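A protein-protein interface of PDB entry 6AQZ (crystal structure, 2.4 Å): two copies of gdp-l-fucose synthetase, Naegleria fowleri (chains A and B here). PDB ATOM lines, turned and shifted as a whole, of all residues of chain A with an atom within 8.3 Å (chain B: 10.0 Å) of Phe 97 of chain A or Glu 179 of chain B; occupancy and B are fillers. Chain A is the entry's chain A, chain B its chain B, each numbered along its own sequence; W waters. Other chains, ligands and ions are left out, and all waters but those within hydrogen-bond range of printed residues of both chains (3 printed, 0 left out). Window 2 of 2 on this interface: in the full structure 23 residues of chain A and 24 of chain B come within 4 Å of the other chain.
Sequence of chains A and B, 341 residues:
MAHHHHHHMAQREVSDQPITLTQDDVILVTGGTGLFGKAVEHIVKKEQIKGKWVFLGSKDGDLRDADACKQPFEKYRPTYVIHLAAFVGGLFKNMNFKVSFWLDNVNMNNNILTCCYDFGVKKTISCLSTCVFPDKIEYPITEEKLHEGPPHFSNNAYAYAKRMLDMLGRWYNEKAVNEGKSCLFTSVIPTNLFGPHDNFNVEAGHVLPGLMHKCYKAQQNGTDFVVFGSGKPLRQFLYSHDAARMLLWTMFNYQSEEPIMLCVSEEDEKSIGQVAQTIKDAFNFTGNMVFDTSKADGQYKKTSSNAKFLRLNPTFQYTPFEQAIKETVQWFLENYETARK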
ATOM      1  N   PHE A  87      24.028 -10.867  17.912  1.00  0.00           N
ATOM      2  CA  PHE A  87      23.405 -11.974  17.208  1.00  0.00           C
ATOM      3  C   PHE A  87      22.842 -11.407  15.914  1.00  0.00           C
ATOM      4  O   PHE A  87      21.897 -10.618  15.931  1.00  0.00           O
ATOM      5  CB  PHE A  87      22.333 -12.643  18.053  1.00  0.00           C
ATOM      6  CG  PHE A  87      21.542 -13.655  17.307  1.00  0.00           C
ATOM      7  CD1 PHE A  87      22.077 -14.883  17.017  1.00  0.00           C
ATOM      8  CD2 PHE A  87      20.248 -13.369  16.886  1.00  0.00           C
ATOM      9  CE1 PHE A  87      21.345 -15.818  16.316  1.00  0.00           C
ATOM     10  CE2 PHE A  87      19.501 -14.302  16.184  1.00  0.00           C
ATOM     11  CZ  PHE A  87      20.054 -15.525  15.898  1.00  0.00           C
ATOM     12  N   GLY A  89      22.128 -13.316  13.120  1.00  0.00           N
ATOM     13  CA  GLY A  89      21.459 -14.340  12.361  1.00  0.00           C
ATOM     14  C   GLY A  89      22.032 -15.685  12.739  1.00  0.00           C
ATOM     15  O   GLY A  89      23.218 -15.798  13.057  1.00  0.00           O
ATOM     16  N   GLY A  90      21.190 -16.699  12.742  1.00  0.00           N
ATOM     17  CA  GLY A  90      21.628 -18.057  12.936  1.00  0.00           C
ATOM     18  C   GLY A  90      21.741 -18.758  11.603  1.00  0.00           C
ATOM     19  O   GLY A  90      21.224 -18.304  10.584  1.00  0.00           O
ATOM     20  N   PHE A  92      20.410 -21.551  11.030  1.00  0.00           N
ATOM     21  CA  PHE A  92      19.182 -22.307  10.863  1.00  0.00           C
ATOM     22  C   PHE A  92      17.952 -21.425  11.042  1.00  0.00           C
ATOM     23  O   PHE A  92      17.957 -20.449  11.811  1.00  0.00           O
ATOM     24  CB  PHE A  92      19.174 -23.477  11.837  1.00  0.00           C
ATOM     25  CG  PHE A  92      20.429 -24.301  11.758  1.00  0.00           C
ATOM     26  CD1 PHE A  92      20.569 -25.281  10.786  1.00  0.00           C
ATOM     27  CD2 PHE A  92      21.496 -24.050  12.607  1.00  0.00           C
ATOM     28  CE1 PHE A  92      21.731 -26.022  10.694  1.00  0.00           C
ATOM     29  CE2 PHE A  92      22.662 -24.793  12.512  1.00  0.00           C
ATOM     30  CZ  PHE A  92      22.771 -25.784  11.554  1.00  0.00           C
ATOM     31  N   LYS A  93      16.903 -21.784  10.296  1.00  0.00           N
ATOM     32  CA  LYS A  93      15.705 -20.957  10.229  1.00  0.00           C
ATOM     33  C   LYS A  93      15.098 -20.732  11.616  1.00  0.00           C
ATOM     34  O   LYS A  93      14.760 -19.595  11.978  1.00  0.00           O
ATOM     35  CB  LYS A  93      14.697 -21.611   9.273  1.00  0.00           C
ATOM     36  N   ASN A  94      14.988 -21.799  12.420  1.00  0.00           N
ATOM     37  CA  ASN A  94      14.328 -21.749  13.721  1.00  0.00           C
ATOM     38  C   ASN A  94      15.008 -20.808  14.695  1.00  0.00           C
ATOM     39  O   ASN A  94      14.407 -20.467  15.714  1.00  0.00           O
ATOM     40  CB  ASN A  94      14.266 -23.144  14.352  1.00  0.00           C
ATOM     41  N   MET A  95      16.236 -20.386  14.421  1.00  0.00           N
ATOM     42  CA  MET A  95      16.891 -19.408  15.264  1.00  0.00           C
ATOM     43  C   MET A  95      16.717 -17.992  14.749  1.00  0.00           C
ATOM     44  O   MET A  95      17.318 -17.081  15.316  1.00  0.00           O
ATOM     45  CB  MET A  95      18.391 -19.700  15.380  1.00  0.00           C
ATOM     46  CG  MET A  95      18.793 -21.124  15.687  1.00  0.00           C
ATOM     47  SD  MET A  95      20.597 -21.310  15.473  1.00  0.00           S
ATOM     48  CE  MET A  95      20.852 -22.885  16.276  1.00  0.00           C
ATOM     49  N   ASN A  96      15.938 -17.778  13.685  1.00  0.00           N
ATOM     50  CA  ASN A  96      15.902 -16.464  13.046  1.00  0.00           C
ATOM     51  C   ASN A  96      14.532 -15.781  13.088  1.00  0.00           C
ATOM     52  O   ASN A  96      14.343 -14.790  12.376  1.00  0.00           O
ATOM     53  CB  ASN A  96      16.381 -16.569  11.586  1.00  0.00           C
ATOM     54  CG  ASN A  96      17.842 -17.021  11.475  1.00  0.00           C
ATOM     55  OD1 ASN A  96      18.662 -16.725  12.349  1.00  0.00           O
ATOM     56  ND2 ASN A  96      18.163 -17.763  10.409  1.00  0.00           N
ATOM     57  N   PHE A  97      13.574 -16.262  13.887  1.00  0.00           N
ATOM     58  CA  PHE A  97      12.365 -15.471  14.104  1.00  0.00           C
ATOM     59  C   PHE A  97      12.731 -14.117  14.688  1.00  0.00           C
ATOM     60  O   PHE A  97      13.770 -13.958  15.342  1.00  0.00           O
ATOM     61  CB  PHE A  97      11.389 -16.186  15.032  1.00  0.00           C
ATOM     62  CG  PHE A  97      10.730 -17.385  14.409  1.00  0.00           C
ATOM     63  CD1 PHE A  97       9.755 -17.225  13.446  1.00  0.00           C
ATOM     64  CD2 PHE A  97      11.088 -18.670  14.790  1.00  0.00           C
ATOM     65  CE1 PHE A  97       9.131 -18.337  12.863  1.00  0.00           C
ATOM     66  CE2 PHE A  97      10.473 -19.792  14.207  1.00  0.00           C
ATOM     67  CZ  PHE A  97       9.494 -19.619  13.250  1.00  0.00           C
ATOM     68  N   LYS A  98      11.901 -13.111  14.411  1.00  0.00           N
ATOM     69  CA  LYS A  98      12.164 -11.806  15.023  1.00  0.00           C
ATOM     70  C   LYS A  98      12.285 -11.910  16.533  1.00  0.00           C
ATOM     71  O   LYS A  98      13.104 -11.211  17.129  1.00  0.00           O
ATOM     72  CB  LYS A  98      11.088 -10.792  14.639  1.00  0.00           C
ATOM     73  CG  LYS A  98      11.313 -10.210  13.257  1.00  0.00           C
ATOM     74  CD  LYS A  98      10.348  -9.107  12.987  1.00  0.00           C
ATOM     75  CE  LYS A  98      10.557  -8.507  11.635  1.00  0.00           C
ATOM     76  NZ  LYS A  98       9.489  -7.506  11.408  1.00  0.00           N
ATOM     77  N   VAL A  99      11.546 -12.837  17.154  1.00  0.00           N
ATOM     78  CA  VAL A  99      11.639 -13.049  18.599  1.00  0.00           C
ATOM     79  C   VAL A  99      13.087 -13.239  19.024  1.00  0.00           C
ATOM     80  O   VAL A  99      13.582 -12.559  19.933  1.00  0.00           O
ATOM     81  CB  VAL A  99      10.776 -14.260  19.003  1.00  0.00           C
ATOM     82  CG1 VAL A  99      11.177 -14.802  20.341  1.00  0.00           C
ATOM     83  CG2 VAL A  99       9.317 -13.861  19.060  1.00  0.00           C
ATOM     84  N   SER A 100      13.816 -14.101  18.311  1.00  0.00           N
ATOM     85  CA  SER A 100      15.198 -14.377  18.695  1.00  0.00           C
ATOM     86  C   SER A 100      16.087 -13.143  18.522  1.00  0.00           C
ATOM     87  O   SER A 100      16.924 -12.846  19.382  1.00  0.00           O
ATOM     88  CB  SER A 100      15.718 -15.550  17.878  1.00  0.00           C
ATOM     89  OG  SER A 100      15.195 -16.765  18.363  1.00  0.00           O
ATOM     90  N   PHE A 101      15.896 -12.386  17.440  1.00  0.00           N
ATOM     91  CA  PHE A 101      16.713 -11.192  17.251  1.00  0.00           C
ATOM     92  C   PHE A 101      16.516 -10.191  18.379  1.00  0.00           C
ATOM     93  O   PHE A 101      17.448  -9.439  18.703  1.00  0.00           O
ATOM     94  CB  PHE A 101      16.411 -10.528  15.912  1.00  0.00           C
ATOM     95  CG  PHE A 101      17.082 -11.183  14.737  1.00  0.00           C
ATOM     96  CD1 PHE A 101      18.363 -10.812  14.362  1.00  0.00           C
ATOM     97  CD2 PHE A 101      16.424 -12.143  13.991  1.00  0.00           C
ATOM     98  CE1 PHE A 101      18.998 -11.418  13.262  1.00  0.00           C
ATOM     99  CE2 PHE A 101      17.036 -12.740  12.899  1.00  0.00           C
ATOM    100  CZ  PHE A 101      18.324 -12.380  12.535  1.00  0.00           C
ATOM    101  N   TRP A 102      15.301 -10.111  18.950  1.00  0.00           N
ATOM    102  CA  TRP A 102      15.112  -9.248  20.111  1.00  0.00           C
ATOM    103  C   TRP A 102      15.773  -9.854  21.349  1.00  0.00           C
ATOM    104  O   TRP A 102      16.649  -9.239  21.966  1.00  0.00           O
ATOM    105  CB  TRP A 102      13.626  -8.989  20.377  1.00  0.00           C
ATOM    106  CG  TRP A 102      13.436  -8.300  21.688  1.00  0.00           C
ATOM    107  CD1 TRP A 102      12.946  -8.846  22.833  1.00  0.00           C
ATOM    108  CD2 TRP A 102      13.805  -6.948  22.006  1.00  0.00           C
ATOM    109  NE1 TRP A 102      12.970  -7.920  23.839  1.00  0.00           N
ATOM    110  CE2 TRP A 102      13.492  -6.743  23.364  1.00  0.00           C
ATOM    111  CE3 TRP A 102      14.346  -5.886  21.265  1.00  0.00           C
ATOM    112  CZ2 TRP A 102      13.684  -5.505  24.015  1.00  0.00           C
ATOM    113  CZ3 TRP A 102      14.579  -4.675  21.913  1.00  0.00           C
ATOM    114  CH2 TRP A 102      14.229  -4.487  23.278  1.00  0.00           C
ATOM    115  N   LEU A 103      15.389 -11.086  21.703  1.00  0.00           N
ATOM    116  CA  LEU A 103      15.821 -11.680  22.969  1.00  0.00           C
ATOM    117  C   LEU A 103      17.331 -11.875  23.018  1.00  0.00           C
ATOM    118  O   LEU A 103      17.977 -11.485  24.000  1.00  0.00           O
ATOM    119  CB  LEU A 103      15.121 -13.025  23.204  1.00  0.00           C
ATOM    120  CG  LEU A 103      13.601 -12.962  23.301  1.00  0.00           C
ATOM    121  CD1 LEU A 103      12.971 -14.334  23.452  1.00  0.00           C
ATOM    122  CD2 LEU A 103      13.234 -11.998  24.426  1.00  0.00           C
ATOM    123  N   ASP A 104      17.910 -12.492  21.975  1.00  0.00           N
ATOM    124  CA  ASP A 104      19.343 -12.777  21.995  1.00  0.00           C
ATOM    125  C   ASP A 104      20.151 -11.507  22.125  1.00  0.00           C
ATOM    126  O   ASP A 104      21.133 -11.458  22.880  1.00  0.00           O
ATOM    127  CB  ASP A 104      19.759 -13.515  20.731  1.00  0.00           C
ATOM    128  CG  ASP A 104      19.238 -14.925  20.691  1.00  0.00           C
ATOM    129  OD1 ASP A 104      18.580 -15.341  21.673  1.00  0.00           O
ATOM    130  OD2 ASP A 104      19.506 -15.617  19.695  1.00  0.00           O
ATOM    131  N   ALA A 157      13.341  -5.874  15.000  1.00  0.00           N
ATOM    132  CA  ALA A 157      13.775  -6.421  16.287  1.00  0.00           C
ATOM    133  C   ALA A 157      15.267  -6.185  16.502  1.00  0.00           C
ATOM    134  O   ALA A 157      15.697  -5.722  17.563  1.00  0.00           O
ATOM    135  CB  ALA A 157      13.446  -7.915  16.379  1.00  0.00           C
ATOM    136  N   TYR A 158      16.080  -6.532  15.513  1.00  0.00           N
ATOM    137  CA  TYR A 158      17.492  -6.206  15.604  1.00  0.00           C
ATOM    138  C   TYR A 158      17.677  -4.702  15.793  1.00  0.00           C
ATOM    139  O   TYR A 158      18.452  -4.264  16.649  1.00  0.00           O
ATOM    140  CB  TYR A 158      18.195  -6.719  14.343  1.00  0.00           C
ATOM    141  CG  TYR A 158      19.653  -6.408  14.256  1.00  0.00           C
ATOM    142  CD1 TYR A 158      20.583  -7.251  14.843  1.00  0.00           C
ATOM    143  CD2 TYR A 158      20.115  -5.289  13.569  1.00  0.00           C
ATOM    144  CE1 TYR A 158      21.936  -6.999  14.758  1.00  0.00           C
ATOM    145  CE2 TYR A 158      21.478  -5.029  13.478  1.00  0.00           C
ATOM    146  CZ  TYR A 158      22.378  -5.894  14.084  1.00  0.00           C
ATOM    147  OH  TYR A 158      23.726  -5.669  14.020  1.00  0.00           O
ATOM    148  N   TYR B 117       3.843 -17.916  25.065  1.00  0.00           N
ATOM    149  CA  TYR B 117       3.961 -18.615  23.796  1.00  0.00           C
ATOM    150  C   TYR B 117       4.313 -20.089  24.013  1.00  0.00           C
ATOM    151  O   TYR B 117       3.699 -20.975  23.415  1.00  0.00           O
ATOM    152  CB  TYR B 117       5.003 -17.941  22.912  1.00  0.00           C
ATOM    153  CG  TYR B 117       5.058 -18.554  21.526  1.00  0.00           C
ATOM    154  CD1 TYR B 117       4.231 -18.092  20.523  1.00  0.00           C
ATOM    155  CD2 TYR B 117       5.918 -19.625  21.232  1.00  0.00           C
ATOM    156  CE1 TYR B 117       4.237 -18.656  19.268  1.00  0.00           C
ATOM    157  CE2 TYR B 117       5.943 -20.195  19.969  1.00  0.00           C
ATOM    158  CZ  TYR B 117       5.100 -19.695  18.978  1.00  0.00           C
ATOM    159  OH  TYR B 117       5.076 -20.209  17.689  1.00  0.00           O
ATOM    160  N   ASP B 118       5.312 -20.367  24.859  1.00  0.00           N
ATOM    161  CA  ASP B 118       5.774 -21.738  25.049  1.00  0.00           C
ATOM    162  C   ASP B 118       4.709 -22.642  25.657  1.00  0.00           C
ATOM    163  O   ASP B 118       4.632 -23.826  25.318  1.00  0.00           O
ATOM    164  CB  ASP B 118       7.032 -21.749  25.913  1.00  0.00           C
ATOM    165  CG  ASP B 118       8.247 -21.217  25.174  1.00  0.00           C
ATOM    166  OD1 ASP B 118       8.124 -20.998  23.951  1.00  0.00           O
ATOM    167  OD2 ASP B 118       9.309 -21.008  25.811  1.00  0.00           O
ATOM    168  N   GLY B 120       1.509 -22.323  25.275  1.00  0.00           N
ATOM    169  CA  GLY B 120       0.285 -22.362  24.481  1.00  0.00           C
ATOM    170  C   GLY B 120      -0.882 -21.563  25.023  1.00  0.00           C
ATOM    171  O   GLY B 120      -2.029 -21.999  24.895  1.00  0.00           O
ATOM    172  N   LEU B 168       7.300  -6.956  21.427  1.00  0.00           N
ATOM    173  CA  LEU B 168       7.505  -8.378  21.644  1.00  0.00           C
ATOM    174  C   LEU B 168       6.222  -9.161  21.419  1.00  0.00           C
ATOM    175  O   LEU B 168       6.269 -10.302  20.934  1.00  0.00           O
ATOM    176  CB  LEU B 168       8.056  -8.641  23.033  1.00  0.00           C
ATOM    177  CG  LEU B 168       8.432 -10.114  23.235  1.00  0.00           C
ATOM    178  CD1 LEU B 168       9.363 -10.609  22.060  1.00  0.00           C
ATOM    179  CD2 LEU B 168       9.163 -10.295  24.574  1.00  0.00           C
ATOM    180  N   ARG B 170       3.845  -8.296  19.166  1.00  0.00           N
ATOM    181  CA  ARG B 170       3.721  -8.408  17.714  1.00  0.00           C
ATOM    182  C   ARG B 170       4.683  -9.459  17.158  1.00  0.00           C
ATOM    183  O   ARG B 170       4.331 -10.207  16.235  1.00  0.00           O
ATOM    184  CB  ARG B 170       4.004  -7.062  17.045  1.00  0.00           C
ATOM    185  CG  ARG B 170       3.139  -5.926  17.499  1.00  0.00           C
ATOM    186  CD  ARG B 170       3.639  -4.593  16.926  1.00  0.00           C
ATOM    187  NE  ARG B 170       2.918  -3.453  17.495  1.00  0.00           N
ATOM    188  CZ  ARG B 170       1.903  -2.840  16.899  1.00  0.00           C
ATOM    189  NH1 ARG B 170       1.501  -3.251  15.703  1.00  0.00           N
ATOM    190  NH2 ARG B 170       1.300  -1.811  17.492  1.00  0.00           N
ATOM    191  N   TRP B 171       5.903  -9.528  17.710  1.00  0.00           N
ATOM    192  CA  TRP B 171       6.871 -10.499  17.218  1.00  0.00           C
ATOM    193  C   TRP B 171       6.438 -11.934  17.537  1.00  0.00           C
ATOM    194  O   TRP B 171       6.652 -12.844  16.722  1.00  0.00           O
ATOM    195  CB  TRP B 171       8.271 -10.170  17.781  1.00  0.00           C
ATOM    196  CG  TRP B 171       8.808  -8.832  17.236  1.00  0.00           C
ATOM    197  CD1 TRP B 171       8.564  -8.313  16.004  1.00  0.00           C
ATOM    198  CD2 TRP B 171       9.625  -7.859  17.921  1.00  0.00           C
ATOM    199  NE1 TRP B 171       9.183  -7.101  15.865  1.00  0.00           N
ATOM    200  CE2 TRP B 171       9.835  -6.792  17.030  1.00  0.00           C
ATOM    201  CE3 TRP B 171      10.200  -7.789  19.194  1.00  0.00           C
ATOM    202  CZ2 TRP B 171      10.601  -5.664  17.371  1.00  0.00           C
ATOM    203  CZ3 TRP B 171      10.962  -6.665  19.532  1.00  0.00           C
ATOM    204  CH2 TRP B 171      11.161  -5.630  18.618  1.00  0.00           C
ATOM    205  N   TYR B 172       5.819 -12.162  18.701  1.00  0.00           N
ATOM    206  CA  TYR B 172       5.320 -13.504  18.998  1.00  0.00           C
ATOM    207  C   TYR B 172       4.115 -13.836  18.143  1.00  0.00           C
ATOM    208  O   TYR B 172       3.908 -15.004  17.815  1.00  0.00           O
ATOM    209  CB  TYR B 172       5.010 -13.679  20.495  1.00  0.00           C
ATOM    210  CG  TYR B 172       6.193 -14.229  21.269  1.00  0.00           C
ATOM    211  CD1 TYR B 172       6.767 -15.466  20.931  1.00  0.00           C
ATOM    212  CD2 TYR B 172       6.793 -13.483  22.283  1.00  0.00           C
ATOM    213  CE1 TYR B 172       7.882 -15.962  21.619  1.00  0.00           C
ATOM    214  CE2 TYR B 172       7.904 -13.962  22.975  1.00  0.00           C
ATOM    215  CZ  TYR B 172       8.449 -15.196  22.635  1.00  0.00           C
ATOM    216  OH  TYR B 172       9.544 -15.649  23.335  1.00  0.00           O
ATOM    217  N   ASN B 173       3.332 -12.832  17.740  1.00  0.00           N
ATOM    218  CA  ASN B 173       2.261 -13.103  16.782  1.00  0.00           C
ATOM    219  C   ASN B 173       2.825 -13.576  15.450  1.00  0.00           C
ATOM    220  O   ASN B 173       2.281 -14.496  14.834  1.00  0.00           O
ATOM    221  CB  ASN B 173       1.388 -11.862  16.560  1.00  0.00           C
ATOM    222  CG  ASN B 173       0.484 -11.542  17.760  1.00  0.00           C
ATOM    223  OD1 ASN B 173       0.076 -12.424  18.511  1.00  0.00           O
ATOM    224  ND2 ASN B 173       0.174 -10.271  17.931  1.00  0.00           N
ATOM    225  N   GLU B 174       3.911 -12.948  14.982  1.00  0.00           N
ATOM    226  CA  GLU B 174       4.536 -13.399  13.752  1.00  0.00           C
ATOM    227  C   GLU B 174       4.989 -14.840  13.870  1.00  0.00           C
ATOM    228  O   GLU B 174       4.779 -15.640  12.955  1.00  0.00           O
ATOM    229  CB  GLU B 174       5.731 -12.536  13.389  1.00  0.00           C
ATOM    230  CG  GLU B 174       5.425 -11.219  12.797  1.00  0.00           C
ATOM    231  CD  GLU B 174       6.702 -10.516  12.370  1.00  0.00           C
ATOM    232  OE1 GLU B 174       6.791  -9.275  12.524  1.00  0.00           O
ATOM    233  OE2 GLU B 174       7.620 -11.221  11.881  1.00  0.00           O
ATOM    234  N   LYS B 175       5.609 -15.190  14.995  1.00  0.00           N
ATOM    235  CA  LYS B 175       6.069 -16.560  15.177  1.00  0.00           C
ATOM    236  C   LYS B 175       4.889 -17.526  15.217  1.00  0.00           C
ATOM    237  O   LYS B 175       4.921 -18.583  14.581  1.00  0.00           O
ATOM    238  CB  LYS B 175       6.910 -16.654  16.454  1.00  0.00           C
ATOM    239  CG  LYS B 175       7.558 -17.999  16.655  1.00  0.00           C
ATOM    240  CD  LYS B 175       8.377 -18.076  17.928  1.00  0.00           C
ATOM    241  CE  LYS B 175       9.101 -19.429  18.016  1.00  0.00           C
ATOM    242  NZ  LYS B 175      10.035 -19.435  19.192  1.00  0.00           N
ATOM    243  N   ALA B 176       3.820 -17.162  15.921  1.00  0.00           N
ATOM    244  CA  ALA B 176       2.653 -18.041  15.978  1.00  0.00           C
ATOM    245  C   ALA B 176       2.066 -18.267  14.595  1.00  0.00           C
ATOM    246  O   ALA B 176       1.694 -19.394  14.247  1.00  0.00           O
ATOM    247  CB  ALA B 176       1.588 -17.468  16.901  1.00  0.00           C
ATOM    248  N   VAL B 177       1.974 -17.205  13.796  1.00  0.00           N
ATOM    249  CA  VAL B 177       1.455 -17.362  12.450  1.00  0.00           C
ATOM    250  C   VAL B 177       2.331 -18.330  11.679  1.00  0.00           C
ATOM    251  O   VAL B 177       1.834 -19.243  11.017  1.00  0.00           O
ATOM    252  CB  VAL B 177       1.343 -15.993  11.754  1.00  0.00           C
ATOM    253  CG1 VAL B 177       1.207 -16.196  10.252  1.00  0.00           C
ATOM    254  CG2 VAL B 177       0.131 -15.192  12.309  1.00  0.00           C
ATOM    255  N   ASN B 178       3.653 -18.186  11.821  1.00  0.00           N
ATOM    256  CA  ASN B 178       4.612 -18.986  11.071  1.00  0.00           C
ATOM    257  C   ASN B 178       4.566 -20.460  11.455  1.00  0.00           C
ATOM    258  O   ASN B 178       4.713 -21.335  10.595  1.00  0.00           O
ATOM    259  CB  ASN B 178       6.006 -18.429  11.304  1.00  0.00           C
ATOM    260  CG  ASN B 178       6.666 -18.031  10.038  1.00  0.00           C
ATOM    261  OD1 ASN B 178       7.472 -18.783   9.488  1.00  0.00           O
ATOM    262  ND2 ASN B 178       6.303 -16.856   9.526  1.00  0.00           N
ATOM    263  N   GLU B 179       4.363 -20.752  12.728  1.00  0.00           N
ATOM    264  CA  GLU B 179       4.324 -22.115  13.233  1.00  0.00           C
ATOM    265  C   GLU B 179       2.907 -22.680  13.319  1.00  0.00           C
ATOM    266  O   GLU B 179       2.726 -23.810  13.793  1.00  0.00           O
ATOM    267  CB  GLU B 179       4.997 -22.149  14.604  1.00  0.00           C
ATOM    268  CG  GLU B 179       6.469 -21.814  14.525  1.00  0.00           C
ATOM    269  CD  GLU B 179       7.226 -22.210  15.766  1.00  0.00           C
ATOM    270  OE1 GLU B 179       6.650 -22.086  16.876  1.00  0.00           O
ATOM    271  OE2 GLU B 179       8.372 -22.708  15.624  1.00  0.00           O
ATOM    272  N   GLY B 180       1.900 -21.932  12.876  1.00  0.00           N
ATOM    273  CA  GLY B 180       0.539 -22.424  12.970  1.00  0.00           C
ATOM    274  C   GLY B 180       0.010 -22.571  14.376  1.00  0.00           C
ATOM    275  O   GLY B 180      -0.935 -23.328  14.583  1.00  0.00           O
ATOM    276  N   LYS B 181       0.632 -21.929  15.358  1.00  0.00           N
ATOM    277  CA  LYS B 181       0.159 -21.958  16.736  1.00  0.00           C
ATOM    278  C   LYS B 181      -0.938 -20.928  16.944  1.00  0.00           C
ATOM    279  O   LYS B 181      -0.937 -19.866  16.311  1.00  0.00           O
ATOM    280  CB  LYS B 181       1.333 -21.697  17.680  1.00  0.00           C
ATOM    281  CG  LYS B 181       1.141 -22.098  19.125  1.00  0.00           C
ATOM    282  CD  LYS B 181       2.508 -22.229  19.810  1.00  0.00           C
ATOM    283  CE  LYS B 181       2.376 -22.932  21.153  1.00  0.00           C
ATOM    284  NZ  LYS B 181       3.669 -23.119  21.846  1.00  0.00           N
ATOM    285  N   SER B 182      -1.866 -21.227  17.866  1.00  0.00           N
ATOM    286  CA  SER B 182      -2.991 -20.322  18.184  1.00  0.00           C
ATOM    287  C   SER B 182      -2.664 -19.563  19.467  1.00  0.00           C
ATOM    288  O   SER B 182      -3.138 -19.874  20.556  1.00  0.00           O
ATOM    289  CB  SER B 182      -4.315 -21.081  18.330  1.00  0.00           C
ATOM    290  OG  SER B 182      -4.816 -21.524  17.085  1.00  0.00           O
ATOM    291  N   CYS B 183      -1.821 -18.555  19.315  1.00  0.00           N
ATOM    292  CA  CYS B 183      -1.395 -17.678  20.393  1.00  0.00           C
ATOM    293  C   CYS B 183      -1.636 -16.270  19.894  1.00  0.00           C
ATOM    294  O   CYS B 183      -1.126 -15.896  18.830  1.00  0.00           O
ATOM    295  CB  CYS B 183       0.080 -17.885  20.756  1.00  0.00           C
ATOM    296  SG  CYS B 183       0.365 -19.426  21.634  1.00  0.00           S
HETATM  297  O   HOH W   1       9.578 -13.441  12.895  1.00  0.00           O
HETATM  298  O   HOH W   2      12.356 -17.753  18.895  1.00  0.00           O
HETATM  299  O   HOH W   3       9.190 -13.601  15.569  1.00  0.00           O
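OE1 of Glu 179 of chain B lies within hydrogen-bond range of OH of Tyr 117 of chain B (2.6 Å).
Water W1 lies within hydrogen-bond range of the backbone NH (N) of Lys 98 of chain A and the side-chain carboxylate (OE2) of Glu 174 of chain B. Water W2 bridges the side-chain amino group of Lys 175 of chain B (2.9 Å) and the side-chain hydroxyl of Ser 100 of chain A (3.1 Å). Water W3 lies within hydrogen-bond range of the backbone carbonyl oxygen (O) of Trp 171 of chain B, the backbone NH (N) of Val 99 of chain A and the backbone NH (N) of Lys 98 of chain A.
CD2 of Phe 97 of chain A touches CE of Lys 175 of chain B, 3.9 Å away. Phe 97 of chain A touches Asn 178 of chain B. CE2 of Phe 97 of chain A touches OE2 of Glu 179 of chain B (3.9 Å). Lys 98 of chain A touches Trp 171 of chain B. Trp 171 of chain B touches Val 99 of chain A. Tyr 172 of chain B touches Val 99 of chain A. CB of Trp 102 of chain A touches CZ3 of Trp 171 of chain B, at 3.6 Å. Leu 103 of chain A touches Tyr 172 of chain B (CD1 to OH, 3.7 Å). CA of Ala 157 of chain A touches CZ2 of Trp 171 of chain B, 3.4 Å away.
The side-chain carboxylate (OE1) of Glu 174 of chain B lies within salt-bridge range of the side-chain amino group (NZ) of Lys 98 of chain A.
No position is printed for both chains.
No residue of chain B comes within 4 Å of Asn 94 of chain A. Asn 96 of chain A touches none of the printed residues of chain B. Phe 97 of chain A touches just these residues of chain B: Lys 175 (3.9 Å), Asn 178 (3.5 Å) and Glu 179 (3.9 Å). Printed residues of chain B within 4 Å of Lys 98 of chain A: Trp 171 (3.6 Å) and Glu 174 (3.4 Å). Of chain B, only Trp 171 (3.7 Å) and Tyr 172 (3.5 Å) come within 4 Å of Val 99 of chain A. No residue of chain B comes within 4 Å of Ser 100 of chain A. Of the printed residues of chain B, Trp 102 of chain A touches Trp 171. Leu 168 of chain B touches none of the printed residues of chain A. Printed residues of chain A within 4 Å of Tyr 172 of chain B: Val 99 (3.5 Å) and Leu 103 (3.7 Å). Printed residues of chain A within 4 Å of Lys 175 of chain B: Phe 97 (3.9 Å). Printed residues of chain A within 4 Å of Asn 178 of chain B: Phe 97 (3.5 Å). Glu 179 of chain B touches one residue of chain A. No residue of chain A comes within 4 Å of Gly 180 of chain B. The nearest residue of chain A that does not touch Glu 179 of chain B is Asn 94 of chain A (6.0 Å).
Of the 18 printed residues of chain A, 6 touch a printed residue of chain B. Hydrophobic or aromatic side chains of chain A that line the printed part of chain B: Phe 97, Val 99, Trp 102, Leu 103 and Ala 157. Hydrophobic or aromatic side chains of chain B within 4 Å of the printed part of chain A: Trp 171 and Tyr 172. Among the printed residues, 10 pairs touch across the chains. Among the printed residues, Asp or Glu carboxylates within 4 Å of a Lys or Arg side-chain nitrogen of the other chain: Lys 98 of chain A with Glu 174 of chain B (3.4 Å).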
